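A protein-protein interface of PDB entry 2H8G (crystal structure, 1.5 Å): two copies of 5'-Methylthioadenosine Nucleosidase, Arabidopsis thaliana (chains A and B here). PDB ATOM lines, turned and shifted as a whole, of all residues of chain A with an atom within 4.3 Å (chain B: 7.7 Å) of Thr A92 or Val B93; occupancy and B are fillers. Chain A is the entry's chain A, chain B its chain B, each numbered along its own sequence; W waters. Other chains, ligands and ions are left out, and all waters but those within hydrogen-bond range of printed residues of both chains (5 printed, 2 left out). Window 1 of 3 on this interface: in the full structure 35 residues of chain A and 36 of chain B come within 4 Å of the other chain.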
ATOM      1  N   GLY A  91      -7.198 -23.956   2.016  1.00  0.00           N
ATOM      2  CA  GLY A  91      -7.423 -24.276   0.618  1.00  0.00           C
ATOM      3  C   GLY A  91      -8.871 -24.156   0.189  1.00  0.00           C
ATOM      4  O   GLY A  91      -9.781 -24.087   1.017  1.00  0.00           O
ATOM      5  N   THR A  92      -9.081 -24.171  -1.123  1.00  0.00           N
ATOM      6  CA  THR A  92     -10.417 -24.013  -1.684  1.00  0.00           C
ATOM      7  C   THR A  92     -11.389 -25.154  -1.428  1.00  0.00           C
ATOM      8  O   THR A  92     -12.574 -24.919  -1.222  1.00  0.00           O
ATOM      9  CB  THR A  92     -10.353 -23.763  -3.214  1.00  0.00           C
ATOM     10  OG1 THR A  92      -9.719 -24.870  -3.868  1.00  0.00           O
ATOM     11  CG2 THR A  92      -9.586 -22.489  -3.505  1.00  0.00           C
ATOM     12  N   VAL A  93     -10.910 -26.390  -1.435  1.00  0.00           N
ATOM     13  CA  VAL A  93     -11.830 -27.496  -1.215  1.00  0.00           C
ATOM     14  C   VAL A  93     -12.476 -27.480   0.172  1.00  0.00           C
ATOM     15  O   VAL A  93     -13.700 -27.507   0.279  1.00  0.00           O
ATOM     16  CB  VAL A  93     -11.147 -28.847  -1.521  1.00  0.00           C
ATOM     17  CG1 VAL A  93     -11.965 -30.000  -0.968  1.00  0.00           C
ATOM     18  CG2 VAL A  93     -11.019 -29.000  -3.036  1.00  0.00           C
ATOM     19  N   PRO A  94     -11.678 -27.419   1.254  1.00  0.00           N
ATOM     20  CA  PRO A  94     -12.328 -27.398   2.573  1.00  0.00           C
ATOM     21  C   PRO A  94     -13.202 -26.158   2.790  1.00  0.00           C
ATOM     22  O   PRO A  94     -14.258 -26.230   3.431  1.00  0.00           O
ATOM     23  CB  PRO A  94     -11.151 -27.444   3.540  1.00  0.00           C
ATOM     24  CG  PRO A  94     -10.125 -28.216   2.784  1.00  0.00           C
ATOM     25  CD  PRO A  94     -10.227 -27.631   1.388  1.00  0.00           C
ATOM     26  N   ALA A  95     -12.763 -25.018   2.262  1.00  0.00           N
ATOM     27  CA  ALA A  95     -13.529 -23.783   2.402  1.00  0.00           C
ATOM     28  C   ALA A  95     -14.877 -23.919   1.708  1.00  0.00           C
ATOM     29  O   ALA A  95     -15.894 -23.481   2.228  1.00  0.00           O
ATOM     30  CB  ALA A  95     -12.755 -22.616   1.807  1.00  0.00           C
ATOM     31  N   SER A  96     -14.881 -24.533   0.531  1.00  0.00           N
ATOM     32  CA  SER A  96     -16.128 -24.692  -0.201  1.00  0.00           C
ATOM     33  C   SER A  96     -17.066 -25.626   0.551  1.00  0.00           C
ATOM     34  O   SER A  96     -18.270 -25.382   0.606  1.00  0.00           O
ATOM     35  CB  SER A  96     -15.862 -25.226  -1.620  1.00  0.00           C
ATOM     36  OG  SER A  96     -15.538 -26.605  -1.634  1.00  0.00           O
ATOM     37  N   PHE A 138     -10.184 -16.651  -9.641  1.00  0.00           N
ATOM     38  CA  PHE A 138      -9.193 -17.709  -9.391  1.00  0.00           C
ATOM     39  C   PHE A 138      -8.048 -17.440 -10.365  1.00  0.00           C
ATOM     40  O   PHE A 138      -8.294 -17.019 -11.495  1.00  0.00           O
ATOM     41  CB  PHE A 138      -9.699 -19.112  -9.752  1.00  0.00           C
ATOM     42  CG  PHE A 138     -10.725 -19.681  -8.816  1.00  0.00           C
ATOM     43  CD1 PHE A 138     -12.077 -19.516  -9.072  1.00  0.00           C
ATOM     44  CD2 PHE A 138     -10.339 -20.443  -7.717  1.00  0.00           C
ATOM     45  CE1 PHE A 138     -13.037 -20.110  -8.255  1.00  0.00           C
ATOM     46  CE2 PHE A 138     -11.289 -21.039  -6.893  1.00  0.00           C
ATOM     47  CZ  PHE A 138     -12.639 -20.876  -7.162  1.00  0.00           C
ATOM     48  N   THR A 177      -7.685 -15.850  -5.942  1.00  0.00           N
ATOM     49  CA  THR A 177      -7.540 -17.082  -5.179  1.00  0.00           C
ATOM     50  C   THR A 177      -6.832 -18.211  -5.909  1.00  0.00           C
ATOM     51  O   THR A 177      -7.020 -18.403  -7.109  1.00  0.00           O
ATOM     52  CB  THR A 177      -8.945 -17.598  -4.779  1.00  0.00           C
ATOM     53  OG1 THR A 177      -9.587 -16.616  -3.955  1.00  0.00           O
ATOM     54  CG2 THR A 177      -8.862 -18.935  -4.049  1.00  0.00           C
ATOM     55  N   ASP A 179      -4.762 -22.305  -4.796  1.00  0.00           N
ATOM     56  CA  ASP A 179      -4.421 -23.207  -3.704  1.00  0.00           C
ATOM     57  C   ASP A 179      -2.959 -23.276  -3.303  1.00  0.00           C
ATOM     58  O   ASP A 179      -2.577 -24.141  -2.512  1.00  0.00           O
ATOM     59  CB  ASP A 179      -4.932 -24.611  -3.998  1.00  0.00           C
ATOM     60  CG  ASP A 179      -6.404 -24.740  -3.722  1.00  0.00           C
ATOM     61  OD1 ASP A 179      -7.207 -24.623  -4.669  1.00  0.00           O
ATOM     62  OD2 ASP A 179      -6.756 -24.935  -2.542  1.00  0.00           O
ATOM     63  N   MET A 201      -6.157 -18.017  -0.507  1.00  0.00           N
ATOM     64  CA  MET A 201      -6.338 -19.413  -0.861  1.00  0.00           C
ATOM     65  C   MET A 201      -7.754 -19.966  -0.724  1.00  0.00           C
ATOM     66  O   MET A 201      -7.953 -21.162  -0.927  1.00  0.00           O
ATOM     67  CB  MET A 201      -5.367 -20.273  -0.037  1.00  0.00           C
ATOM     68  CG  MET A 201      -3.903 -19.993  -0.337  1.00  0.00           C
ATOM     69  SD  MET A 201      -2.750 -20.729   0.841  1.00  0.00           S
ATOM     70  CE  MET A 201      -2.987 -22.440   0.504  1.00  0.00           C
ATOM     71  N   ALA A 205     -13.623 -19.615  -3.879  1.00  0.00           N
ATOM     72  CA  ALA A 205     -14.373 -20.847  -3.673  1.00  0.00           C
ATOM     73  C   ALA A 205     -15.558 -20.560  -2.760  1.00  0.00           C
ATOM     74  O   ALA A 205     -16.651 -21.091  -2.958  1.00  0.00           O
ATOM     75  CB  ALA A 205     -13.476 -21.919  -3.060  1.00  0.00           C
ATOM     76  N   TYR A 208     -18.024 -18.911  -4.865  1.00  0.00           N
ATOM     77  CA  TYR A 208     -18.666 -19.862  -5.766  1.00  0.00           C
ATOM     78  C   TYR A 208     -19.860 -20.527  -5.075  1.00  0.00           C
ATOM     79  O   TYR A 208     -20.964 -20.570  -5.619  1.00  0.00           O
ATOM     80  CB  TYR A 208     -17.668 -20.935  -6.210  1.00  0.00           C
ATOM     81  CG  TYR A 208     -18.284 -21.982  -7.102  1.00  0.00           C
ATOM     82  CD1 TYR A 208     -18.645 -21.679  -8.413  1.00  0.00           C
ATOM     83  CD2 TYR A 208     -18.555 -23.260  -6.622  1.00  0.00           C
ATOM     84  CE1 TYR A 208     -19.262 -22.619  -9.223  1.00  0.00           C
ATOM     85  CE2 TYR A 208     -19.176 -24.213  -7.428  1.00  0.00           C
ATOM     86  CZ  TYR A 208     -19.525 -23.881  -8.727  1.00  0.00           C
ATOM     87  OH  TYR A 208     -20.137 -24.806  -9.537  1.00  0.00           O
ATOM     88  N   TRP B  62     -26.695 -29.149  -9.952  1.00  0.00           N
ATOM     89  CA  TRP B  62     -26.290 -30.549  -9.902  1.00  0.00           C
ATOM     90  C   TRP B  62     -27.348 -31.482 -10.476  1.00  0.00           C
ATOM     91  O   TRP B  62     -28.555 -31.260 -10.317  1.00  0.00           O
ATOM     92  CB  TRP B  62     -25.968 -30.942  -8.459  1.00  0.00           C
ATOM     93  CG  TRP B  62     -24.963 -30.034  -7.815  1.00  0.00           C
ATOM     94  CD1 TRP B  62     -24.117 -29.167  -8.448  1.00  0.00           C
ATOM     95  CD2 TRP B  62     -24.667 -29.932  -6.417  1.00  0.00           C
ATOM     96  NE1 TRP B  62     -23.315 -28.532  -7.533  1.00  0.00           N
ATOM     97  CE2 TRP B  62     -23.629 -28.983  -6.279  1.00  0.00           C
ATOM     98  CE3 TRP B  62     -25.176 -30.551  -5.267  1.00  0.00           C
ATOM     99  CZ2 TRP B  62     -23.087 -28.638  -5.034  1.00  0.00           C
ATOM    100  CZ3 TRP B  62     -24.637 -30.208  -4.028  1.00  0.00           C
ATOM    101  CH2 TRP B  62     -23.602 -29.259  -3.925  1.00  0.00           C
ATOM    102  N   PRO B  79     -21.870 -32.301 -11.510  1.00  0.00           N
ATOM    103  CA  PRO B  79     -21.941 -30.915 -11.038  1.00  0.00           C
ATOM    104  C   PRO B  79     -22.845 -30.025 -11.886  1.00  0.00           C
ATOM    105  O   PRO B  79     -23.184 -28.911 -11.484  1.00  0.00           O
ATOM    106  CB  PRO B  79     -20.478 -30.473 -11.050  1.00  0.00           C
ATOM    107  CG  PRO B  79     -19.900 -31.262 -12.183  1.00  0.00           C
ATOM    108  CD  PRO B  79     -20.515 -32.631 -11.992  1.00  0.00           C
ATOM    109  N   SER B  89     -19.370 -27.894 -14.965  1.00  0.00           N
ATOM    110  CA  SER B  89     -18.635 -27.279 -13.870  1.00  0.00           C
ATOM    111  C   SER B  89     -17.544 -28.227 -13.394  1.00  0.00           C
ATOM    112  O   SER B  89     -17.656 -28.849 -12.338  1.00  0.00           O
ATOM    113  CB  SER B  89     -19.588 -26.945 -12.722  1.00  0.00           C
ATOM    114  OG  SER B  89     -20.598 -26.045 -13.162  1.00  0.00           O
ATOM    115  N   VAL B  90     -16.483 -28.325 -14.187  1.00  0.00           N
ATOM    116  CA  VAL B  90     -15.366 -29.207 -13.875  1.00  0.00           C
ATOM    117  C   VAL B  90     -14.482 -28.644 -12.762  1.00  0.00           C
ATOM    118  O   VAL B  90     -14.657 -27.508 -12.330  1.00  0.00           O
ATOM    119  CB  VAL B  90     -14.500 -29.477 -15.141  1.00  0.00           C
ATOM    120  CG1 VAL B  90     -15.363 -30.143 -16.223  1.00  0.00           C
ATOM    121  CG2 VAL B  90     -13.898 -28.172 -15.667  1.00  0.00           C
ATOM    122  N   GLY B  91     -13.546 -29.452 -12.281  1.00  0.00           N
ATOM    123  CA  GLY B  91     -12.668 -28.955 -11.239  1.00  0.00           C
ATOM    124  C   GLY B  91     -12.893 -29.550  -9.867  1.00  0.00           C
ATOM    125  O   GLY B  91     -13.910 -30.197  -9.599  1.00  0.00           O
ATOM    126  N   THR B  92     -11.948 -29.280  -8.972  1.00  0.00           N
ATOM    127  CA  THR B  92     -11.987 -29.836  -7.631  1.00  0.00           C
ATOM    128  C   THR B  92     -13.085 -29.335  -6.710  1.00  0.00           C
ATOM    129  O   THR B  92     -13.636 -30.119  -5.941  1.00  0.00           O
ATOM    130  CB  THR B  92     -10.625 -29.653  -6.918  1.00  0.00           C
ATOM    131  OG1 THR B  92     -10.330 -28.258  -6.793  1.00  0.00           O
ATOM    132  CG2 THR B  92      -9.512 -30.358  -7.708  1.00  0.00           C
ATOM    133  N   VAL B  93     -13.419 -28.049  -6.772  1.00  0.00           N
ATOM    134  CA  VAL B  93     -14.450 -27.532  -5.888  1.00  0.00           C
ATOM    135  C   VAL B  93     -15.823 -28.171  -6.152  1.00  0.00           C
ATOM    136  O   VAL B  93     -16.418 -28.724  -5.231  1.00  0.00           O
ATOM    137  CB  VAL B  93     -14.503 -25.990  -5.935  1.00  0.00           C
ATOM    138  CG1 VAL B  93     -15.763 -25.483  -5.267  1.00  0.00           C
ATOM    139  CG2 VAL B  93     -13.270 -25.427  -5.208  1.00  0.00           C
ATOM    140  N   PRO B  94     -16.336 -28.133  -7.401  1.00  0.00           N
ATOM    141  CA  PRO B  94     -17.644 -28.764  -7.616  1.00  0.00           C
ATOM    142  C   PRO B  94     -17.623 -30.275  -7.339  1.00  0.00           C
ATOM    143  O   PRO B  94     -18.589 -30.833  -6.813  1.00  0.00           O
ATOM    144  CB  PRO B  94     -17.940 -28.466  -9.086  1.00  0.00           C
ATOM    145  CG  PRO B  94     -17.218 -27.187  -9.329  1.00  0.00           C
ATOM    146  CD  PRO B  94     -15.903 -27.414  -8.611  1.00  0.00           C
ATOM    147  N   ALA B  95     -16.531 -30.943  -7.702  1.00  0.00           N
ATOM    148  CA  ALA B  95     -16.431 -32.381  -7.476  1.00  0.00           C
ATOM    149  C   ALA B  95     -16.500 -32.672  -5.982  1.00  0.00           C
ATOM    150  O   ALA B  95     -17.189 -33.601  -5.562  1.00  0.00           O
ATOM    151  CB  ALA B  95     -15.124 -32.920  -8.054  1.00  0.00           C
ATOM    152  N   SER B  96     -15.798 -31.879  -5.180  1.00  0.00           N
ATOM    153  CA  SER B  96     -15.808 -32.108  -3.740  1.00  0.00           C
ATOM    154  C   SER B  96     -17.206 -31.888  -3.160  1.00  0.00           C
ATOM    155  O   SER B  96     -17.653 -32.646  -2.303  1.00  0.00           O
ATOM    156  CB  SER B  96     -14.787 -31.200  -3.034  1.00  0.00           C
ATOM    157  OG  SER B  96     -15.195 -29.844  -3.002  1.00  0.00           O
ATOM    158  N   LEU B  97     -17.896 -30.860  -3.643  1.00  0.00           N
ATOM    159  CA  LEU B  97     -19.235 -30.544  -3.163  1.00  0.00           C
ATOM    160  C   LEU B  97     -20.246 -31.642  -3.445  1.00  0.00           C
ATOM    161  O   LEU B  97     -20.984 -32.051  -2.547  1.00  0.00           O
ATOM    162  CB  LEU B  97     -19.723 -29.232  -3.791  1.00  0.00           C
ATOM    163  CG  LEU B  97     -19.008 -27.957  -3.332  1.00  0.00           C
ATOM    164  CD1 LEU B  97     -19.361 -26.799  -4.248  1.00  0.00           C
ATOM    165  CD2 LEU B  97     -19.405 -27.645  -1.896  1.00  0.00           C
ATOM    166  N   ILE B  98     -20.296 -32.117  -4.687  1.00  0.00           N
ATOM    167  CA  ILE B  98     -21.266 -33.155  -5.011  1.00  0.00           C
ATOM    168  C   ILE B  98     -20.932 -34.486  -4.357  1.00  0.00           C
ATOM    169  O   ILE B  98     -21.833 -35.284  -4.091  1.00  0.00           O
ATOM    170  CB  ILE B  98     -21.446 -33.347  -6.540  1.00  0.00           C
ATOM    171  CG1 ILE B  98     -20.153 -33.843  -7.188  1.00  0.00           C
ATOM    172  CG2 ILE B  98     -21.901 -32.039  -7.166  1.00  0.00           C
ATOM    173  CD1 ILE B  98     -20.290 -34.078  -8.697  1.00  0.00           C
ATOM    174  N   THR B  99     -19.650 -34.724  -4.087  1.00  0.00           N
ATOM    175  CA  THR B  99     -19.230 -35.953  -3.424  1.00  0.00           C
ATOM    176  C   THR B  99     -19.745 -35.878  -1.988  1.00  0.00           C
ATOM    177  O   THR B  99     -20.329 -36.828  -1.473  1.00  0.00           O
ATOM    178  CB  THR B  99     -17.690 -36.092  -3.407  1.00  0.00           C
ATOM    179  OG1 THR B  99     -17.212 -36.229  -4.750  1.00  0.00           O
ATOM    180  CG2 THR B  99     -17.265 -37.317  -2.600  1.00  0.00           C
ATOM    181  N   PHE B 138      -2.293 -34.221  -5.362  1.00  0.00           N
ATOM    182  CA  PHE B 138      -2.545 -32.932  -6.006  1.00  0.00           C
ATOM    183  C   PHE B 138      -1.172 -32.423  -6.445  1.00  0.00           C
ATOM    184  O   PHE B 138      -0.182 -32.617  -5.734  1.00  0.00           O
ATOM    185  CB  PHE B 138      -3.070 -31.872  -5.034  1.00  0.00           C
ATOM    186  CG  PHE B 138      -4.487 -32.064  -4.583  1.00  0.00           C
ATOM    187  CD1 PHE B 138      -4.764 -32.718  -3.389  1.00  0.00           C
ATOM    188  CD2 PHE B 138      -5.542 -31.488  -5.291  1.00  0.00           C
ATOM    189  CE1 PHE B 138      -6.063 -32.786  -2.895  1.00  0.00           C
ATOM    190  CE2 PHE B 138      -6.845 -31.554  -4.802  1.00  0.00           C
ATOM    191  CZ  PHE B 138      -7.107 -32.198  -3.604  1.00  0.00           C
ATOM    192  N   ARG B 141      -1.212 -27.631  -5.252  1.00  0.00           N
ATOM    193  CA  ARG B 141      -1.489 -27.048  -3.944  1.00  0.00           C
ATOM    194  C   ARG B 141      -0.125 -26.993  -3.258  1.00  0.00           C
ATOM    195  O   ARG B 141       0.217 -27.847  -2.435  1.00  0.00           O
ATOM    196  CB  ARG B 141      -2.476 -27.910  -3.151  1.00  0.00           C
ATOM    197  CG  ARG B 141      -3.777 -28.217  -3.904  1.00  0.00           C
ATOM    198  CD  ARG B 141      -4.930 -28.539  -2.958  1.00  0.00           C
ATOM    199  NE  ARG B 141      -4.591 -29.564  -1.974  1.00  0.00           N
ATOM    200  CZ  ARG B 141      -5.408 -29.966  -1.005  1.00  0.00           C
ATOM    201  NH1 ARG B 141      -6.618 -29.432  -0.886  1.00  0.00           N
ATOM    202  NH2 ARG B 141      -5.016 -30.896  -0.144  1.00  0.00           N
ATOM    203  N   TYR B 151       0.287 -31.674   3.324  1.00  0.00           N
ATOM    204  CA  TYR B 151      -1.162 -31.515   3.309  1.00  0.00           C
ATOM    205  C   TYR B 151      -1.620 -31.119   1.905  1.00  0.00           C
ATOM    206  O   TYR B 151      -2.600 -31.656   1.384  1.00  0.00           O
ATOM    207  CB  TYR B 151      -1.577 -30.442   4.315  1.00  0.00           C
ATOM    208  CG  TYR B 151      -2.984 -29.931   4.123  1.00  0.00           C
ATOM    209  CD1 TYR B 151      -4.085 -30.667   4.554  1.00  0.00           C
ATOM    210  CD2 TYR B 151      -3.210 -28.714   3.483  1.00  0.00           C
ATOM    211  CE1 TYR B 151      -5.387 -30.203   4.352  1.00  0.00           C
ATOM    212  CE2 TYR B 151      -4.500 -28.242   3.274  1.00  0.00           C
ATOM    213  CZ  TYR B 151      -5.580 -28.988   3.709  1.00  0.00           C
ATOM    214  OH  TYR B 151      -6.855 -28.518   3.493  1.00  0.00           O
ATOM    215  N   ASP B 179      -6.338 -28.120 -10.894  1.00  0.00           N
ATOM    216  CA  ASP B 179      -7.461 -27.436 -11.514  1.00  0.00           C
ATOM    217  C   ASP B 179      -7.216 -26.841 -12.887  1.00  0.00           C
ATOM    218  O   ASP B 179      -8.071 -26.131 -13.423  1.00  0.00           O
ATOM    219  CB  ASP B 179      -8.014 -26.373 -10.573  1.00  0.00           C
ATOM    220  CG  ASP B 179      -8.958 -26.966  -9.562  1.00  0.00           C
ATOM    221  OD1 ASP B 179      -8.540 -27.208  -8.417  1.00  0.00           O
ATOM    222  OD2 ASP B 179     -10.122 -27.223  -9.931  1.00  0.00           O
ATOM    223  N   MET B 201      -8.583 -33.440 -13.170  1.00  0.00           N
ATOM    224  CA  MET B 201      -8.951 -32.218 -12.463  1.00  0.00           C
ATOM    225  C   MET B 201      -9.888 -32.392 -11.271  1.00  0.00           C
ATOM    226  O   MET B 201     -10.322 -31.400 -10.696  1.00  0.00           O
ATOM    227  CB  MET B 201      -9.559 -31.224 -13.464  1.00  0.00           C
ATOM    228  CG  MET B 201      -8.614 -30.892 -14.625  1.00  0.00           C
ATOM    229  SD  MET B 201      -9.392 -29.971 -15.983  1.00  0.00           S
ATOM    230  CE  MET B 201     -10.487 -31.213 -16.706  1.00  0.00           C
ATOM    231  N   GLU B 202     -10.184 -33.629 -10.877  1.00  0.00           N
ATOM    232  CA  GLU B 202     -11.095 -33.845  -9.744  1.00  0.00           C
ATOM    233  C   GLU B 202     -10.699 -34.913  -8.719  1.00  0.00           C
ATOM    234  O   GLU B 202     -11.003 -34.778  -7.532  1.00  0.00           O
ATOM    235  CB  GLU B 202     -12.504 -34.218 -10.239  1.00  0.00           C
ATOM    236  CG  GLU B 202     -13.233 -33.175 -11.067  1.00  0.00           C
ATOM    237  CD  GLU B 202     -12.861 -33.223 -12.536  1.00  0.00           C
ATOM    238  OE1 GLU B 202     -12.515 -34.322 -13.027  1.00  0.00           O
ATOM    239  OE2 GLU B 202     -12.939 -32.165 -13.191  1.00  0.00           O
ATOM    240  N   ALA B 205      -9.519 -34.516  -4.993  1.00  0.00           N
ATOM    241  CA  ALA B 205     -10.539 -33.827  -4.211  1.00  0.00           C
ATOM    242  C   ALA B 205     -11.639 -34.801  -3.810  1.00  0.00           C
ATOM    243  O   ALA B 205     -12.159 -34.745  -2.693  1.00  0.00           O
ATOM    244  CB  ALA B 205     -11.125 -32.661  -5.015  1.00  0.00           C
ATOM    245  N   VAL B 209     -12.640 -35.883   0.203  1.00  0.00           N
ATOM    246  CA  VAL B 209     -13.976 -35.927   0.786  1.00  0.00           C
ATOM    247  C   VAL B 209     -14.354 -37.340   1.225  1.00  0.00           C
ATOM    248  O   VAL B 209     -14.906 -37.528   2.307  1.00  0.00           O
ATOM    249  CB  VAL B 209     -15.043 -35.398  -0.209  1.00  0.00           C
ATOM    250  CG1 VAL B 209     -16.426 -35.455   0.425  1.00  0.00           C
ATOM    251  CG2 VAL B 209     -14.713 -33.972  -0.609  1.00  0.00           C
HETATM  252  O   HOH W   1      -8.161 -27.327  -2.273  1.00  0.00           O
HETATM  253  O   HOH W   2      -8.140 -27.848  -5.026  1.00  0.00           O
HETATM  254  O   HOH W   3     -20.930 -23.809 -11.849  1.00  0.00           O
HETATM  255  O   HOH W   4     -10.045 -24.763  -6.600  1.00  0.00           O
HETATM  256  O   HOH W   5     -21.556 -27.230  -9.400  1.00  0.00           O
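Water W3 bridges OG of Ser B89 (2.6 Å) and OH of Tyr A208 (2.6 Å). Water W4 lies within hydrogen-bond range of the side-chain hydroxyl of Thr A92 (2.8 Å), the side-chain carboxylate of Asp B179 (3.4 Å) and the side-chain carboxylate of Asp A179 (3.4 Å). Water W1 lies within hydrogen-bond range of OD2 of Asp A179 (2.8 Å), NH1 of Arg B141 (3.0 Å), N of Val A93 (3.0 Å) and OG1 of Thr A92 (3.3 Å). Water W5 lies within hydrogen-bond range of the side-chain hydroxyl (OH) of Tyr A208 (2.8 Å), the indole nitrogen (NE1) of Trp B62 (2.9 Å) and the backbone carbonyl oxygen (O) of Pro B79 (3.1 Å). Water W2 lies within hydrogen-bond range of OG1 of Thr B92 (2.8 Å), OD1 of Asp A179 (3.4 Å) and OD1 of Asp B179 (3.5 Å).
Hydrophobic or aromatic side chains of chain A that line the printed part of chain B: Val A93, Pro A94 and Tyr A208. Along chain B the printed residues that touch a printed residue of chain A span positions 89 to 151. Among the printed residues, 11 pairs touch across the chains. Among the printed residues, no Asp or Glu carboxylate lies within 4 Å of a Lys or Arg side-chain nitrogen of the other chain.
Thr A92 touches Val B93, and with the chains exchanged Val A93 touches Thr B92. Val A93 touches Ser B96, and with the chains exchanged Ser A96 touches Val B93. Ser A96 touches its own counterpart, Ser B96. Of the 11 pairs that touch across the chains among the printed residues, 5 have their exchanged pair printed and touching as well.
Among the printed residues, pairs that only touch across the chains: Thr A92 with Val B93 (3.8 Å), Val A93 with Thr B92 (3.9 Å), Val A93 with Ser B96 (3.7 Å), Pro A94 with Tyr B151 (3.4 Å), Ser A96 with Val B93 (3.7 Å), Ser A96 with Ser B96 (3.5 Å), Ser A96 with Leu B97 (3.6 Å), Asp A179 with Arg B141 (3.4 Å), Tyr A208 with Ser B89 (3.9 Å), Tyr A208 with Val B93 (3.8 Å) and Tyr A208 with Pro B94 (3.8 Å).
OG of Ser A96 lies close to O of Thr A92 (3.4 Å). The backbone carbonyl oxygen (O) of Val A93 lies within hydrogen-bond range of the side-chain hydroxyl (OG) of Ser A96 (2.8 Å). The backbone carbonyl oxygen (O) of Thr B92 lies close to the side-chain hydroxyl (OG) of Ser B96 (3.3 Å). OG1 of Thr B92 is in hydrogen-bond range of OD1 of Asp B179 (2.6 Å). The backbone carbonyl oxygen (O) of Met B201 is in hydrogen-bond range of the backbone NH (N) of Thr B92 (3.2 Å). O of Val B93 lies within hydrogen-bond range of OG of Ser B96, at 2.8 Å.
Thr A92 touches just one residue of chain B: Val B93. Of chain A, only Thr A92 (3.8 Å), Ser A96 (3.7 Å) and Tyr A208 (3.8 Å) come within 4 Å of Val B93. Printed residues of chain A within 4 Å of Ser B96: Val A93 and Ser A96. Of the printed residues of chain B, Val A93 touches Thr B92 (3.9 Å) and Ser B96 (3.7 Å). Of the printed residues of chain A, Tyr B151 touches Pro A94 (3.4 Å). Of the printed residues of chain B, Pro A94 touches Tyr B151 (3.4 Å). Met B201 touches none of the printed residues of chain A. Ile B98 touches none of the printed residues of chain A.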
